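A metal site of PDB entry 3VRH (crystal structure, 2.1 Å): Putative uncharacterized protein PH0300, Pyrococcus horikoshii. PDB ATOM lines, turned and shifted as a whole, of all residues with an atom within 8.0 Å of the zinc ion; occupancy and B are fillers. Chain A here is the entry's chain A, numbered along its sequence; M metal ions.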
ATOM      1  N   LYS A   2     -25.921 -35.522   1.326  1.00  0.00           N
ATOM      2  CA  LYS A   2     -26.858 -34.679   2.065  1.00  0.00           C
ATOM      3  C   LYS A   2     -26.121 -33.529   2.740  1.00  0.00           C
ATOM      4  O   LYS A   2     -24.919 -33.604   2.985  1.00  0.00           O
ATOM      5  CB  LYS A   2     -27.661 -35.501   3.065  1.00  0.00           C
ATOM      6  CG  LYS A   2     -28.638 -36.486   2.398  1.00  0.00           C
ATOM      7  CD  LYS A   2     -29.600 -35.769   1.434  1.00  0.00           C
ATOM      8  CE  LYS A   2     -30.318 -36.735   0.474  1.00  0.00           C
ATOM      9  NZ  LYS A   2     -31.058 -36.019  -0.625  1.00  0.00           N
ATOM     10  N   CYS A   3     -26.863 -32.469   3.036  1.00  0.00           N
ATOM     11  CA  CYS A   3     -26.286 -31.303   3.661  1.00  0.00           C
ATOM     12  C   CYS A   3     -25.733 -31.642   5.044  1.00  0.00           C
ATOM     13  O   CYS A   3     -26.248 -32.512   5.749  1.00  0.00           O
ATOM     14  CB  CYS A   3     -27.344 -30.184   3.737  1.00  0.00           C
ATOM     15  SG  CYS A   3     -26.788 -28.676   4.562  1.00  0.00           S
ATOM     16  N   LYS A   4     -24.666 -30.946   5.424  1.00  0.00           N
ATOM     17  CA  LYS A   4     -24.081 -31.092   6.747  1.00  0.00           C
ATOM     18  C   LYS A   4     -25.045 -30.661   7.860  1.00  0.00           C
ATOM     19  O   LYS A   4     -24.976 -31.160   8.978  1.00  0.00           O
ATOM     20  CB  LYS A   4     -22.791 -30.286   6.844  1.00  0.00           C
ATOM     21  CG  LYS A   4     -22.029 -30.478   8.153  1.00  0.00           C
ATOM     22  CD  LYS A   4     -20.771 -29.608   8.241  1.00  0.00           C
ATOM     23  CE  LYS A   4     -20.336 -29.391   9.694  1.00  0.00           C
ATOM     24  NZ  LYS A   4     -19.102 -28.531   9.790  1.00  0.00           N
ATOM     25  N   PHE A   5     -25.949 -29.722   7.546  1.00  0.00           N
ATOM     26  CA  PHE A   5     -26.759 -29.083   8.573  1.00  0.00           C
ATOM     27  C   PHE A   5     -28.242 -29.435   8.545  1.00  0.00           C
ATOM     28  O   PHE A   5     -28.999 -29.017   9.435  1.00  0.00           O
ATOM     29  CB  PHE A   5     -26.583 -27.563   8.522  1.00  0.00           C
ATOM     30  CG  PHE A   5     -25.203 -27.115   8.881  1.00  0.00           C
ATOM     31  CD1 PHE A   5     -24.791 -27.090  10.203  1.00  0.00           C
ATOM     32  CD2 PHE A   5     -24.315 -26.710   7.900  1.00  0.00           C
ATOM     33  CE1 PHE A   5     -23.499 -26.680  10.539  1.00  0.00           C
ATOM     34  CE2 PHE A   5     -23.035 -26.297   8.229  1.00  0.00           C
ATOM     35  CZ  PHE A   5     -22.628 -26.283   9.543  1.00  0.00           C
ATOM     36  N   CYS A   6     -28.653 -30.198   7.540  1.00  0.00           N
ATOM     37  CA  CYS A   6     -30.017 -30.682   7.451  1.00  0.00           C
ATOM     38  C   CYS A   6     -30.092 -31.886   6.533  1.00  0.00           C
ATOM     39  O   CYS A   6     -29.059 -32.455   6.136  1.00  0.00           O
ATOM     40  CB  CYS A   6     -30.977 -29.595   6.971  1.00  0.00           C
ATOM     41  SG  CYS A   6     -30.919 -29.191   5.200  1.00  0.00           S
ATOM     42  N   SER A   7     -31.317 -32.267   6.196  1.00  0.00           N
ATOM     43  CA  SER A   7     -31.600 -33.504   5.486  1.00  0.00           C
ATOM     44  C   SER A   7     -31.786 -33.257   3.989  1.00  0.00           C
ATOM     45  O   SER A   7     -32.048 -34.190   3.210  1.00  0.00           O
ATOM     46  CB  SER A   7     -32.828 -34.181   6.121  1.00  0.00           C
ATOM     47  OG  SER A   7     -33.566 -34.948   5.197  1.00  0.00           O
ATOM     48  N   ARG A   8     -31.623 -32.006   3.562  1.00  0.00           N
ATOM     49  CA  ARG A   8     -31.770 -31.636   2.155  1.00  0.00           C
ATOM     50  C   ARG A   8     -30.596 -32.112   1.301  1.00  0.00           C
ATOM     51  O   ARG A   8     -29.491 -32.357   1.810  1.00  0.00           O
ATOM     52  CB  ARG A   8     -31.943 -30.119   1.994  1.00  0.00           C
ATOM     53  CG  ARG A   8     -33.278 -29.584   2.532  1.00  0.00           C
ATOM     54  CD  ARG A   8     -33.424 -28.086   2.333  1.00  0.00           C
ATOM     55  NE  ARG A   8     -34.605 -27.555   3.016  1.00  0.00           N
ATOM     56  CZ  ARG A   8     -34.610 -27.079   4.262  1.00  0.00           C
ATOM     57  NH1 ARG A   8     -33.483 -27.063   4.967  1.00  0.00           N
ATOM     58  NH2 ARG A   8     -35.741 -26.609   4.792  1.00  0.00           N
ATOM     59  N   GLU A   9     -30.848 -32.267   0.000  1.00  0.00           N
ATOM     60  CA  GLU A   9     -29.812 -32.710  -0.934  1.00  0.00           C
ATOM     61  C   GLU A   9     -28.683 -31.669  -1.035  1.00  0.00           C
ATOM     62  O   GLU A   9     -28.930 -30.449  -1.031  1.00  0.00           O
ATOM     63  CB  GLU A   9     -30.408 -32.983  -2.314  1.00  0.00           C
ATOM     64  CG  GLU A   9     -29.485 -33.791  -3.220  1.00  0.00           C
ATOM     65  CD  GLU A   9     -30.167 -34.273  -4.502  1.00  0.00           C
ATOM     66  OE1 GLU A   9     -31.186 -33.669  -4.905  1.00  0.00           O
ATOM     67  OE2 GLU A   9     -29.680 -35.269  -5.099  1.00  0.00           O
ATOM     68  N   ALA A  10     -27.448 -32.148  -1.113  1.00  0.00           N
ATOM     69  CA  ALA A  10     -26.295 -31.266  -1.205  1.00  0.00           C
ATOM     70  C   ALA A  10     -26.375 -30.437  -2.480  1.00  0.00           C
ATOM     71  O   ALA A  10     -26.722 -30.940  -3.530  1.00  0.00           O
ATOM     72  CB  ALA A  10     -25.020 -32.084  -1.174  1.00  0.00           C
ATOM     73  N   TYR A  11     -26.083 -29.155  -2.372  1.00  0.00           N
ATOM     74  CA  TYR A  11     -26.082 -28.292  -3.548  1.00  0.00           C
ATOM     75  C   TYR A  11     -24.668 -28.085  -4.028  1.00  0.00           C
ATOM     76  O   TYR A  11     -24.412 -27.905  -5.225  1.00  0.00           O
ATOM     77  CB  TYR A  11     -26.720 -26.957  -3.205  1.00  0.00           C
ATOM     78  CG  TYR A  11     -26.593 -25.879  -4.272  1.00  0.00           C
ATOM     79  CD1 TYR A  11     -27.221 -26.023  -5.500  1.00  0.00           C
ATOM     80  CD2 TYR A  11     -25.881 -24.710  -4.019  1.00  0.00           C
ATOM     81  CE1 TYR A  11     -27.139 -25.036  -6.461  1.00  0.00           C
ATOM     82  CE2 TYR A  11     -25.792 -23.705  -4.984  1.00  0.00           C
ATOM     83  CZ  TYR A  11     -26.428 -23.875  -6.197  1.00  0.00           C
ATOM     84  OH  TYR A  11     -26.358 -22.901  -7.184  1.00  0.00           O
ATOM     85  N   TYR A  20     -20.611 -30.674   2.744  1.00  0.00           N
ATOM     86  CA  TYR A  20     -21.616 -30.553   1.709  1.00  0.00           C
ATOM     87  C   TYR A  20     -22.699 -29.654   2.253  1.00  0.00           C
ATOM     88  O   TYR A  20     -23.020 -29.723   3.446  1.00  0.00           O
ATOM     89  CB  TYR A  20     -22.191 -31.915   1.344  1.00  0.00           C
ATOM     90  CG  TYR A  20     -21.189 -32.786   0.642  1.00  0.00           C
ATOM     91  CD1 TYR A  20     -21.091 -32.772  -0.744  1.00  0.00           C
ATOM     92  CD2 TYR A  20     -20.314 -33.598   1.358  1.00  0.00           C
ATOM     93  CE1 TYR A  20     -20.164 -33.560  -1.392  1.00  0.00           C
ATOM     94  CE2 TYR A  20     -19.378 -34.389   0.708  1.00  0.00           C
ATOM     95  CZ  TYR A  20     -19.304 -34.355  -0.673  1.00  0.00           C
ATOM     96  OH  TYR A  20     -18.380 -35.144  -1.331  1.00  0.00           O
ATOM     97  N   LEU A  21     -23.240 -28.787   1.396  1.00  0.00           N
ATOM     98  CA  LEU A  21     -24.279 -27.835   1.797  1.00  0.00           C
ATOM     99  C   LEU A  21     -25.418 -27.788   0.796  1.00  0.00           C
ATOM    100  O   LEU A  21     -25.197 -27.794  -0.413  1.00  0.00           O
ATOM    101  CB  LEU A  21     -23.683 -26.428   1.942  1.00  0.00           C
ATOM    102  CG  LEU A  21     -22.612 -26.158   2.991  1.00  0.00           C
ATOM    103  CD1 LEU A  21     -22.174 -24.701   2.894  1.00  0.00           C
ATOM    104  CD2 LEU A  21     -23.111 -26.509   4.400  1.00  0.00           C
ATOM    105  N   CYS A  22     -26.651 -27.709   1.301  1.00  0.00           N
ATOM    106  CA  CYS A  22     -27.808 -27.481   0.464  1.00  0.00           C
ATOM    107  C   CYS A  22     -27.806 -26.022   0.019  1.00  0.00           C
ATOM    108  O   CYS A  22     -26.975 -25.221   0.485  1.00  0.00           O
ATOM    109  CB  CYS A  22     -29.096 -27.770   1.242  1.00  0.00           C
ATOM    110  SG  CYS A  22     -29.525 -26.514   2.463  1.00  0.00           S
ATOM    111  N   GLU A  23     -28.728 -25.674  -0.875  1.00  0.00           N
ATOM    112  CA  GLU A  23     -28.835 -24.323  -1.403  1.00  0.00           C
ATOM    113  C   GLU A  23     -28.901 -23.260  -0.316  1.00  0.00           C
ATOM    114  O   GLU A  23     -28.154 -22.294  -0.355  1.00  0.00           O
ATOM    115  CB  GLU A  23     -30.069 -24.196  -2.292  1.00  0.00           C
ATOM    116  CG  GLU A  23     -29.896 -24.713  -3.696  1.00  0.00           C
ATOM    117  CD  GLU A  23     -30.957 -24.148  -4.626  1.00  0.00           C
ATOM    118  OE1 GLU A  23     -31.277 -24.817  -5.646  1.00  0.00           O
ATOM    119  OE2 GLU A  23     -31.471 -23.043  -4.336  1.00  0.00           O
ATOM    120  N   GLU A  24     -29.800 -23.446   0.655  1.00  0.00           N
ATOM    121  CA  GLU A  24     -30.040 -22.396   1.636  1.00  0.00           C
ATOM    122  C   GLU A  24     -28.883 -22.249   2.611  1.00  0.00           C
ATOM    123  O   GLU A  24     -28.531 -21.138   2.991  1.00  0.00           O
ATOM    124  CB  GLU A  24     -31.350 -22.640   2.384  1.00  0.00           C
ATOM    125  CG  GLU A  24     -32.583 -22.352   1.541  1.00  0.00           C
ATOM    126  CD  GLU A  24     -32.629 -20.920   1.039  1.00  0.00           C
ATOM    127  OE1 GLU A  24     -32.334 -19.997   1.831  1.00  0.00           O
ATOM    128  OE2 GLU A  24     -32.945 -20.705  -0.157  1.00  0.00           O
ATOM    129  N   HIS A  25     -28.292 -23.372   3.001  1.00  0.00           N
ATOM    130  CA  HIS A  25     -27.145 -23.335   3.896  1.00  0.00           C
ATOM    131  C   HIS A  25     -25.890 -22.868   3.182  1.00  0.00           C
ATOM    132  O   HIS A  25     -24.974 -22.343   3.831  1.00  0.00           O
ATOM    133  CB  HIS A  25     -26.923 -24.679   4.611  1.00  0.00           C
ATOM    134  CG  HIS A  25     -27.801 -24.859   5.805  1.00  0.00           C
ATOM    135  ND1 HIS A  25     -28.818 -25.780   5.842  1.00  0.00           N
ATOM    136  CD2 HIS A  25     -27.872 -24.178   6.975  1.00  0.00           C
ATOM    137  CE1 HIS A  25     -29.456 -25.701   6.983  1.00  0.00           C
ATOM    138  NE2 HIS A  25     -28.907 -24.734   7.699  1.00  0.00           N
ATOM    139  N   PHE A  26     -25.828 -23.065   1.870  1.00  0.00           N
ATOM    140  CA  PHE A  26     -24.731 -22.488   1.095  1.00  0.00           C
ATOM    141  C   PHE A  26     -24.848 -20.957   1.052  1.00  0.00           C
ATOM    142  O   PHE A  26     -23.853 -20.249   1.252  1.00  0.00           O
ATOM    143  CB  PHE A  26     -24.694 -23.025  -0.332  1.00  0.00           C
ATOM    144  CG  PHE A  26     -23.779 -22.255  -1.232  1.00  0.00           C
ATOM    145  CD1 PHE A  26     -22.399 -22.283  -1.022  1.00  0.00           C
ATOM    146  CD2 PHE A  26     -24.287 -21.478  -2.256  1.00  0.00           C
ATOM    147  CE1 PHE A  26     -21.549 -21.559  -1.837  1.00  0.00           C
ATOM    148  CE2 PHE A  26     -23.439 -20.755  -3.081  1.00  0.00           C
ATOM    149  CZ  PHE A  26     -22.063 -20.792  -2.868  1.00  0.00           C
ATOM    150  N   GLU A  28     -26.277 -19.025   3.141  1.00  0.00           N
ATOM    151  CA  GLU A  28     -25.910 -18.588   4.485  1.00  0.00           C
ATOM    152  C   GLU A  28     -24.400 -18.606   4.710  1.00  0.00           C
ATOM    153  O   GLU A  28     -23.833 -17.628   5.200  1.00  0.00           O
ATOM    154  CB  GLU A  28     -26.619 -19.471   5.517  1.00  0.00           C
ATOM    155  CG  GLU A  28     -26.223 -19.178   6.951  1.00  0.00           C
ATOM    156  CD  GLU A  28     -27.114 -19.886   7.985  1.00  0.00           C
ATOM    157  OE1 GLU A  28     -27.863 -20.814   7.624  1.00  0.00           O
ATOM    158  OE2 GLU A  28     -27.044 -19.491   9.177  1.00  0.00           O
HETATM  159 ZN    ZN M   1     -28.985 -27.660   4.644  1.00  0.00          ZN
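The side-chain sulfur (SG) of Cys 3 sits close to the backbone NH (N) of Phe 5. N of Cys 3 lies within hydrogen-bond range of O of Arg 8, 2.9 Å away. SG of Cys 22 sits close to N of Glu 24. The side-chain sulfur (SG) of Cys 6 lies close to the backbone NH (N) of Arg 8.
Within 4 Å of the zinc ion: Cys 3, Cys 6, Cys 22 and His 25.
The zinc ion is bound by ND1 of His 25 (2.2 Å), SG of Cys 3 (2.4 Å), SG of Cys 22 (2.5 Å) and SG of Cys 6 (2.5 Å). The zinc ion has four donor atoms within binding distance.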
